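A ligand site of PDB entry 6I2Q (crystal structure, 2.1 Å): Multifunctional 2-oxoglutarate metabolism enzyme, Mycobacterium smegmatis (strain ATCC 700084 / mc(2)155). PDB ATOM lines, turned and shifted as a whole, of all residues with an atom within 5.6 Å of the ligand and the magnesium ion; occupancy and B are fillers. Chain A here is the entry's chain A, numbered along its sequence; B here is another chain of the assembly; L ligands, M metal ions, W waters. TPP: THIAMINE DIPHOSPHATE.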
ATOM      1  N   HIS A 180      21.091  -0.381  23.267  1.00  0.00           N
ATOM      2  CA  HIS A 180      22.268  -1.098  23.795  1.00  0.00           C
ATOM      3  C   HIS A 180      21.991  -2.092  24.934  1.00  0.00           C
ATOM      4  O   HIS A 180      22.672  -3.113  24.980  1.00  0.00           O
ATOM      5  CB  HIS A 180      23.379  -0.120  24.256  1.00  0.00           C
ATOM      6  CG  HIS A 180      22.919   0.901  25.262  1.00  0.00           C
ATOM      7  ND1 HIS A 180      23.106   0.715  26.628  1.00  0.00           N
ATOM      8  CD2 HIS A 180      22.304   2.092  25.073  1.00  0.00           C
ATOM      9  CE1 HIS A 180      22.601   1.781  27.207  1.00  0.00           C
ATOM     10  NE2 HIS A 180      22.094   2.640  26.315  1.00  0.00           N
ATOM     11  N   ARG A 181      21.044  -1.810  25.835  1.00  0.00           N
ATOM     12  CA  ARG A 181      20.825  -2.704  27.013  1.00  0.00           C
ATOM     13  C   ARG A 181      20.571  -4.181  26.635  1.00  0.00           C
ATOM     14  O   ARG A 181      19.615  -4.496  25.938  1.00  0.00           O
ATOM     15  CB  ARG A 181      19.698  -2.202  27.948  1.00  0.00           C
ATOM     16  CG  ARG A 181      19.614  -3.051  29.215  1.00  0.00           C
ATOM     17  CD  ARG A 181      18.626  -2.528  30.222  1.00  0.00           C
ATOM     18  NE  ARG A 181      18.793  -1.096  30.477  1.00  0.00           N
ATOM     19  CZ  ARG A 181      19.718  -0.560  31.275  1.00  0.00           C
ATOM     20  NH1 ARG A 181      20.604  -1.342  31.896  1.00  0.00           N
ATOM     21  NH2 ARG A 181      19.764   0.745  31.453  1.00  0.00           N
ATOM     22  N   SER A 245      23.525   5.790  19.114  1.00  0.00           N
ATOM     23  CA  SER A 245      23.129   5.838  20.528  1.00  0.00           C
ATOM     24  C   SER A 245      21.767   6.526  20.655  1.00  0.00           C
ATOM     25  O   SER A 245      21.111   6.352  21.678  1.00  0.00           O
ATOM     26  CB  SER A 245      24.180   6.558  21.376  1.00  0.00           C
ATOM     27  OG  SER A 245      25.382   5.812  21.345  1.00  0.00           O
ATOM     28  N   HIS A 246      21.358   7.299  19.620  1.00  0.00           N
ATOM     29  CA  HIS A 246      20.071   7.998  19.618  1.00  0.00           C
ATOM     30  C   HIS A 246      18.935   6.984  19.721  1.00  0.00           C
ATOM     31  O   HIS A 246      18.596   6.315  18.753  1.00  0.00           O
ATOM     32  CB  HIS A 246      19.920   8.870  18.343  1.00  0.00           C
ATOM     33  CG  HIS A 246      20.969   9.946  18.229  1.00  0.00           C
ATOM     34  ND1 HIS A 246      20.622  11.278  18.112  1.00  0.00           N
ATOM     35  CD2 HIS A 246      22.313   9.844  18.312  1.00  0.00           C
ATOM     36  CE1 HIS A 246      21.765  11.939  18.082  1.00  0.00           C
ATOM     37  NE2 HIS A 246      22.815  11.120  18.202  1.00  0.00           N
ATOM     38  N   LEU A 247      18.371   6.867  20.924  1.00  0.00           N
ATOM     39  CA  LEU A 247      17.284   5.931  21.250  1.00  0.00           C
ATOM     40  C   LEU A 247      16.084   6.179  20.335  1.00  0.00           C
ATOM     41  O   LEU A 247      15.712   7.317  20.077  1.00  0.00           O
ATOM     42  CB  LEU A 247      16.885   6.080  22.734  1.00  0.00           C
ATOM     43  CG  LEU A 247      18.021   5.818  23.768  1.00  0.00           C
ATOM     44  CD1 LEU A 247      17.612   6.295  25.195  1.00  0.00           C
ATOM     45  CD2 LEU A 247      18.444   4.349  23.769  1.00  0.00           C
ATOM     46  N   GLY A 285      13.089   0.993  25.440  1.00  0.00           N
ATOM     47  CA  GLY A 285      13.150   1.323  26.867  1.00  0.00           C
ATOM     48  C   GLY A 285      11.878   2.079  27.209  1.00  0.00           C
ATOM     49  O   GLY A 285      11.228   2.625  26.317  1.00  0.00           O
ATOM     50  N   ASP A 286      11.487   2.119  28.481  1.00  0.00           N
ATOM     51  CA  ASP A 286      10.222   2.760  28.863  1.00  0.00           C
ATOM     52  C   ASP A 286      10.232   4.277  28.738  1.00  0.00           C
ATOM     53  O   ASP A 286       9.221   4.823  28.294  1.00  0.00           O
ATOM     54  CB  ASP A 286       9.800   2.362  30.295  1.00  0.00           C
ATOM     55  CG  ASP A 286      10.887   2.542  31.362  1.00  0.00           C
ATOM     56  OD1 ASP A 286      11.970   1.970  31.188  1.00  0.00           O
ATOM     57  OD2 ASP A 286      10.632   3.254  32.362  1.00  0.00           O
ATOM     58  N   ALA A 287      11.320   4.965  29.138  1.00  0.00           N
ATOM     59  CA  ALA A 287      11.363   6.437  29.033  1.00  0.00           C
ATOM     60  C   ALA A 287      11.406   6.909  27.577  1.00  0.00           C
ATOM     61  O   ALA A 287      10.647   7.808  27.238  1.00  0.00           O
ATOM     62  CB  ALA A 287      12.537   7.013  29.809  1.00  0.00           C
ATOM     63  N   ALA A 288      12.258   6.283  26.719  1.00  0.00           N
ATOM     64  CA  ALA A 288      12.404   6.665  25.301  1.00  0.00           C
ATOM     65  C   ALA A 288      11.150   6.360  24.488  1.00  0.00           C
ATOM     66  O   ALA A 288      10.836   7.105  23.557  1.00  0.00           O
ATOM     67  CB  ALA A 288      13.579   5.919  24.684  1.00  0.00           C
ATOM     68  N   PHE A 289      10.422   5.260  24.816  1.00  0.00           N
ATOM     69  CA  PHE A 289       9.229   4.866  24.059  1.00  0.00           C
ATOM     70  C   PHE A 289       8.133   5.939  24.164  1.00  0.00           C
ATOM     71  O   PHE A 289       7.419   6.198  23.176  1.00  0.00           O
ATOM     72  CB  PHE A 289       8.709   3.475  24.497  1.00  0.00           C
ATOM     73  CG  PHE A 289       7.750   2.848  23.499  1.00  0.00           C
ATOM     74  CD1 PHE A 289       8.163   2.519  22.217  1.00  0.00           C
ATOM     75  CD2 PHE A 289       6.436   2.555  23.867  1.00  0.00           C
ATOM     76  CE1 PHE A 289       7.293   1.894  21.317  1.00  0.00           C
ATOM     77  CE2 PHE A 289       5.555   1.939  22.952  1.00  0.00           C
ATOM     78  CZ  PHE A 289       5.988   1.623  21.676  1.00  0.00           C
ATOM     79  N   GLN A 292      10.208   9.958  22.652  1.00  0.00           N
ATOM     80  CA  GLN A 292      10.708  10.207  21.297  1.00  0.00           C
ATOM     81  C   GLN A 292       9.582  10.212  20.239  1.00  0.00           C
ATOM     82  O   GLN A 292       8.969   9.177  19.995  1.00  0.00           O
ATOM     83  CB  GLN A 292      11.775   9.126  20.967  1.00  0.00           C
ATOM     84  CG  GLN A 292      13.097   9.315  21.789  1.00  0.00           C
ATOM     85  CD  GLN A 292      13.842  10.570  21.358  1.00  0.00           C
ATOM     86  OE1 GLN A 292      14.124  10.788  20.197  1.00  0.00           O
ATOM     87  NE2 GLN A 292      14.184  11.428  22.292  1.00  0.00           N
ATOM     88  N   VAL A 317      11.340  -2.988  27.344  1.00  0.00           N
ATOM     89  CA  VAL A 317      12.038  -3.437  28.537  1.00  0.00           C
ATOM     90  C   VAL A 317      11.723  -2.349  29.570  1.00  0.00           C
ATOM     91  O   VAL A 317      12.355  -1.275  29.592  1.00  0.00           O
ATOM     92  CB  VAL A 317      13.563  -3.686  28.276  1.00  0.00           C
ATOM     93  CG1 VAL A 317      14.300  -4.062  29.574  1.00  0.00           C
ATOM     94  CG2 VAL A 317      13.751  -4.774  27.199  1.00  0.00           C
ATOM     95  N   ASN A 318      10.631  -2.556  30.295  1.00  0.00           N
ATOM     96  CA  ASN A 318      10.125  -1.543  31.209  1.00  0.00           C
ATOM     97  C   ASN A 318      10.660  -1.751  32.623  1.00  0.00           C
ATOM     98  O   ASN A 318      10.010  -2.370  33.480  1.00  0.00           O
ATOM     99  CB  ASN A 318       8.596  -1.499  31.160  1.00  0.00           C
ATOM    100  CG  ASN A 318       7.965  -0.459  32.044  1.00  0.00           C
ATOM    101  OD1 ASN A 318       8.644   0.390  32.638  1.00  0.00           O
ATOM    102  ND2 ASN A 318       6.656  -0.470  32.130  1.00  0.00           N
ATOM    103  N   ASN A 319      11.837  -1.153  32.883  1.00  0.00           N
ATOM    104  CA  ASN A 319      12.515  -1.250  34.174  1.00  0.00           C
ATOM    105  C   ASN A 319      12.111  -0.123  35.104  1.00  0.00           C
ATOM    106  O   ASN A 319      12.724   0.066  36.153  1.00  0.00           O
ATOM    107  CB  ASN A 319      14.036  -1.313  34.004  1.00  0.00           C
ATOM    108  CG  ASN A 319      14.613  -0.239  33.137  1.00  0.00           C
ATOM    109  OD1 ASN A 319      14.001   0.828  32.878  1.00  0.00           O
ATOM    110  ND2 ASN A 319      15.799  -0.509  32.649  1.00  0.00           N
ATOM    111  N   GLN A 320      11.054   0.632  34.739  1.00  0.00           N
ATOM    112  CA  GLN A 320      10.387   1.657  35.546  1.00  0.00           C
ATOM    113  C   GLN A 320      11.355   2.780  36.000  1.00  0.00           C
ATOM    114  O   GLN A 320      11.198   3.338  37.089  1.00  0.00           O
ATOM    115  CB  GLN A 320       9.698   0.970  36.745  1.00  0.00           C
ATOM    116  CG  GLN A 320       8.869  -0.277  36.285  1.00  0.00           C
ATOM    117  CD  GLN A 320       8.354  -1.078  37.457  1.00  0.00           C
ATOM    118  OE1 GLN A 320       7.513  -0.608  38.222  1.00  0.00           O
ATOM    119  NE2 GLN A 320       8.863  -2.323  37.613  1.00  0.00           N
ATOM    120  N   ILE A 321      12.327   3.103  35.142  1.00  0.00           N
ATOM    121  CA  ILE A 321      13.366   4.121  35.366  1.00  0.00           C
ATOM    122  C   ILE A 321      13.976   4.493  34.000  1.00  0.00           C
ATOM    123  O   ILE A 321      13.949   3.686  33.069  1.00  0.00           O
ATOM    124  CB  ILE A 321      14.438   3.619  36.395  1.00  0.00           C
ATOM    125  CG1 ILE A 321      15.321   4.806  36.905  1.00  0.00           C
ATOM    126  CG2 ILE A 321      15.287   2.411  35.869  1.00  0.00           C
ATOM    127  CD1 ILE A 321      16.167   4.537  38.197  1.00  0.00           C
ATOM    128  N   GLY A 322      14.506   5.705  33.901  1.00  0.00           N
ATOM    129  CA  GLY A 322      15.199   6.215  32.739  1.00  0.00           C
ATOM    130  C   GLY A 322      16.378   6.994  33.271  1.00  0.00           C
ATOM    131  O   GLY A 322      16.233   8.177  33.588  1.00  0.00           O
ATOM    132  N   PHE A 323      17.530   6.306  33.402  1.00  0.00           N
ATOM    133  CA  PHE A 323      18.779   6.818  33.981  1.00  0.00           C
ATOM    134  C   PHE A 323      18.478   7.154  35.484  1.00  0.00           C
ATOM    135  O   PHE A 323      18.388   6.226  36.282  1.00  0.00           O
ATOM    136  CB  PHE A 323      19.396   7.990  33.166  1.00  0.00           C
ATOM    137  CG  PHE A 323      20.845   8.383  33.456  1.00  0.00           C
ATOM    138  CD1 PHE A 323      21.443   8.067  34.673  1.00  0.00           C
ATOM    139  CD2 PHE A 323      21.596   9.094  32.523  1.00  0.00           C
ATOM    140  CE1 PHE A 323      22.778   8.419  34.927  1.00  0.00           C
ATOM    141  CE2 PHE A 323      22.927   9.461  32.790  1.00  0.00           C
ATOM    142  CZ  PHE A 323      23.510   9.109  33.983  1.00  0.00           C
ATOM    143  N   ARG A 384      16.056  -2.594  36.943  1.00  0.00           N
ATOM    144  CA  ARG A 384      17.430  -2.375  36.560  1.00  0.00           C
ATOM    145  C   ARG A 384      18.276  -2.619  37.799  1.00  0.00           C
ATOM    146  O   ARG A 384      18.349  -1.742  38.667  1.00  0.00           O
ATOM    147  CB  ARG A 384      17.580  -0.956  35.973  1.00  0.00           C
ATOM    148  CG  ARG A 384      18.872  -0.735  35.192  1.00  0.00           C
ATOM    149  CD  ARG A 384      19.162   0.761  35.070  1.00  0.00           C
ATOM    150  NE  ARG A 384      19.479   1.347  36.372  1.00  0.00           N
ATOM    151  CZ  ARG A 384      19.357   2.634  36.675  1.00  0.00           C
ATOM    152  NH1 ARG A 384      18.945   3.505  35.762  1.00  0.00           N
ATOM    153  NH2 ARG A 384      19.662   3.066  37.889  1.00  0.00           N
ATOM    154  N   HIS A 388      22.897   3.219  36.429  1.00  0.00           N
ATOM    155  CA  HIS A 388      22.912   3.452  34.998  1.00  0.00           C
ATOM    156  C   HIS A 388      24.289   3.170  34.367  1.00  0.00           C
ATOM    157  O   HIS A 388      24.329   2.686  33.241  1.00  0.00           O
ATOM    158  CB  HIS A 388      22.458   4.855  34.660  1.00  0.00           C
ATOM    159  CG  HIS A 388      22.194   5.048  33.205  1.00  0.00           C
ATOM    160  ND1 HIS A 388      21.039   4.550  32.606  1.00  0.00           N
ATOM    161  CD2 HIS A 388      22.934   5.685  32.267  1.00  0.00           C
ATOM    162  CE1 HIS A 388      21.095   4.924  31.342  1.00  0.00           C
ATOM    163  NE2 HIS A 388      22.231   5.598  31.082  1.00  0.00           N
ATOM    164  N   GLN B 542      17.717  16.270  30.488  1.00  0.00           N
ATOM    165  CA  GLN B 542      17.742  14.866  30.905  1.00  0.00           C
ATOM    166  C   GLN B 542      18.699  14.671  32.063  1.00  0.00           C
ATOM    167  O   GLN B 542      19.900  15.009  31.977  1.00  0.00           O
ATOM    168  CB  GLN B 542      18.064  13.946  29.730  1.00  0.00           C
ATOM    169  CG  GLN B 542      16.881  13.811  28.757  1.00  0.00           C
ATOM    170  CD  GLN B 542      17.329  13.561  27.343  1.00  0.00           C
ATOM    171  OE1 GLN B 542      18.430  13.056  27.099  1.00  0.00           O
ATOM    172  NE2 GLN B 542      16.514  13.918  26.359  1.00  0.00           N
ATOM    173  N   ASP B 543      18.120  14.191  33.187  1.00  0.00           N
ATOM    174  CA  ASP B 543      18.767  13.909  34.480  1.00  0.00           C
ATOM    175  C   ASP B 543      19.522  15.147  35.015  1.00  0.00           C
ATOM    176  O   ASP B 543      20.522  15.015  35.718  1.00  0.00           O
ATOM    177  CB  ASP B 543      19.697  12.667  34.308  1.00  0.00           C
ATOM    178  CG  ASP B 543      18.922  11.483  33.710  1.00  0.00           C
ATOM    179  OD1 ASP B 543      18.131  10.869  34.441  1.00  0.00           O
ATOM    180  OD2 ASP B 543      19.099  11.211  32.493  1.00  0.00           O
ATOM    181  N   LEU B 591      12.169  12.184  28.052  1.00  0.00           N
ATOM    182  CA  LEU B 591      13.279  11.795  27.165  1.00  0.00           C
ATOM    183  C   LEU B 591      12.949  12.270  25.749  1.00  0.00           C
ATOM    184  O   LEU B 591      12.615  11.472  24.856  1.00  0.00           O
ATOM    185  CB  LEU B 591      13.518  10.263  27.224  1.00  0.00           C
ATOM    186  CG  LEU B 591      14.959   9.793  26.996  1.00  0.00           C
ATOM    187  CD1 LEU B 591      15.116   8.338  27.426  1.00  0.00           C
ATOM    188  CD2 LEU B 591      15.419   9.999  25.513  1.00  0.00           C
ATOM    189  N   GLU B 593      14.037  15.724  22.848  1.00  0.00           N
ATOM    190  CA  GLU B 593      14.931  16.839  22.504  1.00  0.00           C
ATOM    191  C   GLU B 593      14.078  17.887  21.788  1.00  0.00           C
ATOM    192  O   GLU B 593      14.046  19.027  22.202  1.00  0.00           O
ATOM    193  CB  GLU B 593      16.161  16.421  21.662  1.00  0.00           C
ATOM    194  CG  GLU B 593      17.210  15.703  22.496  1.00  0.00           C
ATOM    195  CD  GLU B 593      16.971  14.215  22.694  1.00  0.00           C
ATOM    196  OE1 GLU B 593      17.522  13.671  23.671  1.00  0.00           O
ATOM    197  OE2 GLU B 593      16.252  13.587  21.886  1.00  0.00           O
ATOM    198  N   GLN B 617      21.851  15.751  27.292  1.00  0.00           N
ATOM    199  CA  GLN B 617      22.563  14.728  28.081  1.00  0.00           C
ATOM    200  C   GLN B 617      24.035  14.748  27.641  1.00  0.00           C
ATOM    201  O   GLN B 617      24.949  14.813  28.460  1.00  0.00           O
ATOM    202  CB  GLN B 617      21.906  13.342  27.907  1.00  0.00           C
ATOM    203  CG  GLN B 617      22.564  12.285  28.812  1.00  0.00           C
ATOM    204  CD  GLN B 617      21.611  11.654  29.773  1.00  0.00           C
ATOM    205  OE1 GLN B 617      21.156  10.547  29.578  1.00  0.00           O
ATOM    206  NE2 GLN B 617      21.334  12.313  30.855  1.00  0.00           N
ATOM    207  N   PHE B 621      23.076  14.669  21.047  1.00  0.00           N
ATOM    208  CA  PHE B 621      21.664  14.381  20.868  1.00  0.00           C
ATOM    209  C   PHE B 621      20.829  15.640  20.563  1.00  0.00           C
ATOM    210  O   PHE B 621      19.627  15.527  20.302  1.00  0.00           O
ATOM    211  CB  PHE B 621      21.098  13.634  22.106  1.00  0.00           C
ATOM    212  CG  PHE B 621      21.875  12.380  22.454  1.00  0.00           C
ATOM    213  CD1 PHE B 621      22.593  12.279  23.661  1.00  0.00           C
ATOM    214  CD2 PHE B 621      21.915  11.296  21.581  1.00  0.00           C
ATOM    215  CE1 PHE B 621      23.309  11.134  23.977  1.00  0.00           C
ATOM    216  CE2 PHE B 621      22.647  10.144  21.896  1.00  0.00           C
ATOM    217  CZ  PHE B 621      23.347  10.063  23.086  1.00  0.00           C
ATOM    218  N   HIS B 661      29.022  10.561  21.663  1.00  0.00           N
ATOM    219  CA  HIS B 661      29.383  11.013  23.009  1.00  0.00           C
ATOM    220  C   HIS B 661      30.611  11.903  22.934  1.00  0.00           C
ATOM    221  O   HIS B 661      31.461  11.845  23.813  1.00  0.00           O
ATOM    222  CB  HIS B 661      29.618   9.793  23.940  1.00  0.00           C
ATOM    223  CG  HIS B 661      28.365   8.997  24.138  1.00  0.00           C
ATOM    224  ND1 HIS B 661      28.005   7.993  23.259  1.00  0.00           N
ATOM    225  CD2 HIS B 661      27.366   9.187  25.026  1.00  0.00           C
ATOM    226  CE1 HIS B 661      26.830   7.567  23.668  1.00  0.00           C
ATOM    227  NE2 HIS B 661      26.410   8.252  24.733  1.00  0.00           N
HETATM  228  N1' TPP L   1      18.473  11.150  23.865  1.00  0.00           N
HETATM  229  C2' TPP L   1      18.535  10.217  22.896  1.00  0.00           C
HETATM  230  CM2 TPP L   1      17.671  10.413  21.699  1.00  0.00           C
HETATM  231  N3' TPP L   1      19.311   9.126  22.931  1.00  0.00           N
HETATM  232  C4' TPP L   1      20.071   8.911  24.031  1.00  0.00           C
HETATM  233  N4' TPP L   1      20.909   7.875  23.996  1.00  0.00           N
HETATM  234  C5' TPP L   1      20.028   9.826  25.137  1.00  0.00           C
HETATM  235  C6' TPP L   1      19.222  10.927  24.955  1.00  0.00           C
HETATM  236  C7' TPP L   1      20.779   9.614  26.421  1.00  0.00           C
HETATM  237  N3  TPP L   1      20.293   8.452  27.215  1.00  0.00           N
HETATM  238  C2  TPP L   1      20.931   7.297  27.273  1.00  0.00           C
HETATM  239  S1  TPP L   1      20.174   6.191  28.279  1.00  0.00           S
HETATM  240  C5  TPP L   1      18.937   7.324  28.652  1.00  0.00           C
HETATM  241  C4  TPP L   1      19.148   8.507  28.013  1.00  0.00           C
HETATM  242  CM4 TPP L   1      18.363   9.760  28.168  1.00  0.00           C
HETATM  243  C6  TPP L   1      17.742   6.883  29.459  1.00  0.00           C
HETATM  244  C7  TPP L   1      17.051   5.695  28.825  1.00  0.00           C
HETATM  245  O7  TPP L   1      15.838   5.397  29.547  1.00  0.00           O
HETATM  246  PA  TPP L   1      14.909   4.160  29.004  1.00  0.00           P
HETATM  247  O1A TPP L   1      13.882   3.848  30.124  1.00  0.00           O
HETATM  248  O2A TPP L   1      14.484   4.441  27.632  1.00  0.00           O
HETATM  249  O3A TPP L   1      15.934   2.952  28.957  1.00  0.00           O
HETATM  250  PB  TPP L   1      16.870   2.166  29.984  1.00  0.00           P
HETATM  251  O1B TPP L   1      16.205   2.264  31.376  1.00  0.00           O
HETATM  252  O2B TPP L   1      18.253   2.718  29.978  1.00  0.00           O
HETATM  253  O3B TPP L   1      16.768   0.713  29.537  1.00  0.00           O
HETATM  254 MG    MG M   1      13.948   2.310  31.420  1.00  0.00          MG
HETATM  255  O   HOH W   1      16.685   0.460  26.847  1.00  0.00           O
HETATM  256  O   HOH W   2      23.309   8.454  29.196  1.00  0.00           O
HETATM  257  O   HOH W   3      15.737   2.982  25.643  1.00  0.00           O
HETATM  258  O   HOH W   4      14.093   0.646  30.062  1.00  0.00           O
HETATM  259  O   HOH W   5      17.962   3.567  33.056  1.00  0.00           O
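N of Asp 286 lies close to O1A of the ligand (3.4 Å). The side-chain carboxylate (OE1) of Glu 593 of chain B is in hydrogen-bond range of a nitrogen (N1') of the ligand, at 2.7 Å. The backbone carbonyl oxygen (O) of Ser 245 sits at hydrogen-bond distance from a nitrogen (N4') of the ligand (2.8 Å). NE of Arg 181 lies within salt-bridge range of O3B of the ligand. O1A of the ligand sits close to N of Ala 287, 3.0 Å away. N of Ala 288 is in hydrogen-bond range of O2A of the ligand, at 3.0 Å. A nitrogen (N3') of the ligand lies within hydrogen-bond range of the backbone NH (N) of Leu 247 (3.2 Å). A ring nitrogen (NE2) of His 388 lies close to a sulfur (S1) of the ligand (3.5 Å).
OD1 of Asn 318 lies close to OD2 of Asp 286, 3.5 Å away. The side-chain amide nitrogen (NE2) of Gln 542 of chain B sits at hydrogen-bond distance from the side-chain carboxylate (OE1) of Glu 593 of chain B, 2.9 Å away. OE2 of Glu 593 of chain B lies within hydrogen-bond range of NE2 of Gln 292 (3.0 Å). O of Gln 542 of chain B lies within hydrogen-bond range of NE2 of Gln 617 of chain B, 3.3 Å away. The side-chain amide nitrogen of Gln 617 of chain B is in hydrogen-bond range of the side-chain carboxylate of Asp 543 of chain B (3.0 Å). The side-chain amide nitrogen (NE2) of Gln 292 sits at hydrogen-bond distance from the backbone carbonyl oxygen (O) of Leu 591 of chain B (3.0 Å). The backbone carbonyl oxygen (O) of Phe 323 sits at hydrogen-bond distance from the guanidinium group (NH1) of Arg 384.
The side-chain amide oxygen of Gln 617 of chain B lies close to a nitrogen (N3) of the ligand (3.3 Å). Residues that only touch the ligand: Gln 542 of chain B (3.1 Å), Gly 322 (3.4 Å), Phe 621 of chain B (3.4 Å), Gly 285 (3.5 Å), Leu 591 of chain B (3.6 Å), His 246 (3.6 Å), Gln 292 (3.7 Å) and Phe 323 (3.99 Å). Within 4 Å of the ligand: Arg 181, Ser 245, His 246, Leu 247, Gly 285, Asp 286, Ala 287, Ala 288, Gln 292, Asn 319, Ile 321, Gly 322, Phe 323, His 388, Gln 542 of chain B, Leu 591 of chain B, Glu 593 of chain B, Gln 617 of chain B and Phe 621 of chain B. The nearest printed residue that does not touch the ligand is His 180 (4.5 Å).
Three residues have an atom within 4 Å of the magnesium ion: Asp 286, Asn 319 and Ile 321.
An oxygen (O1A) of the ligand is bound to the magnesium ion. OD1 of Asp 286 binds the magnesium ion, at 2.0 Å. OD1 of Asn 319 binds the magnesium ion (2.1 Å). O of Ile 321 binds the magnesium ion (2.1 Å). Water W4 is bound to the magnesium ion. The magnesium ion is bound by O1B of the ligand (2.3 Å).
Water W4 lies within hydrogen-bond range of O of Val 317 (2.6 Å), O3B of the ligand (2.7 Å), ND2 of Asn 319 (3.3 Å) and N of Asp 286 (3.4 Å). Water W5 lies within hydrogen-bond range of N of Phe 323 (2.8 Å), NH1 of Arg 384 (2.9 Å), O2B of the ligand (3.2 Å) and ND1 of His 388 (3.3 Å). Water W3 lies within hydrogen-bond range of an oxygen (O2A) of the ligand (2.8 Å) and the backbone NH of Gly 285 (3.3 Å).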
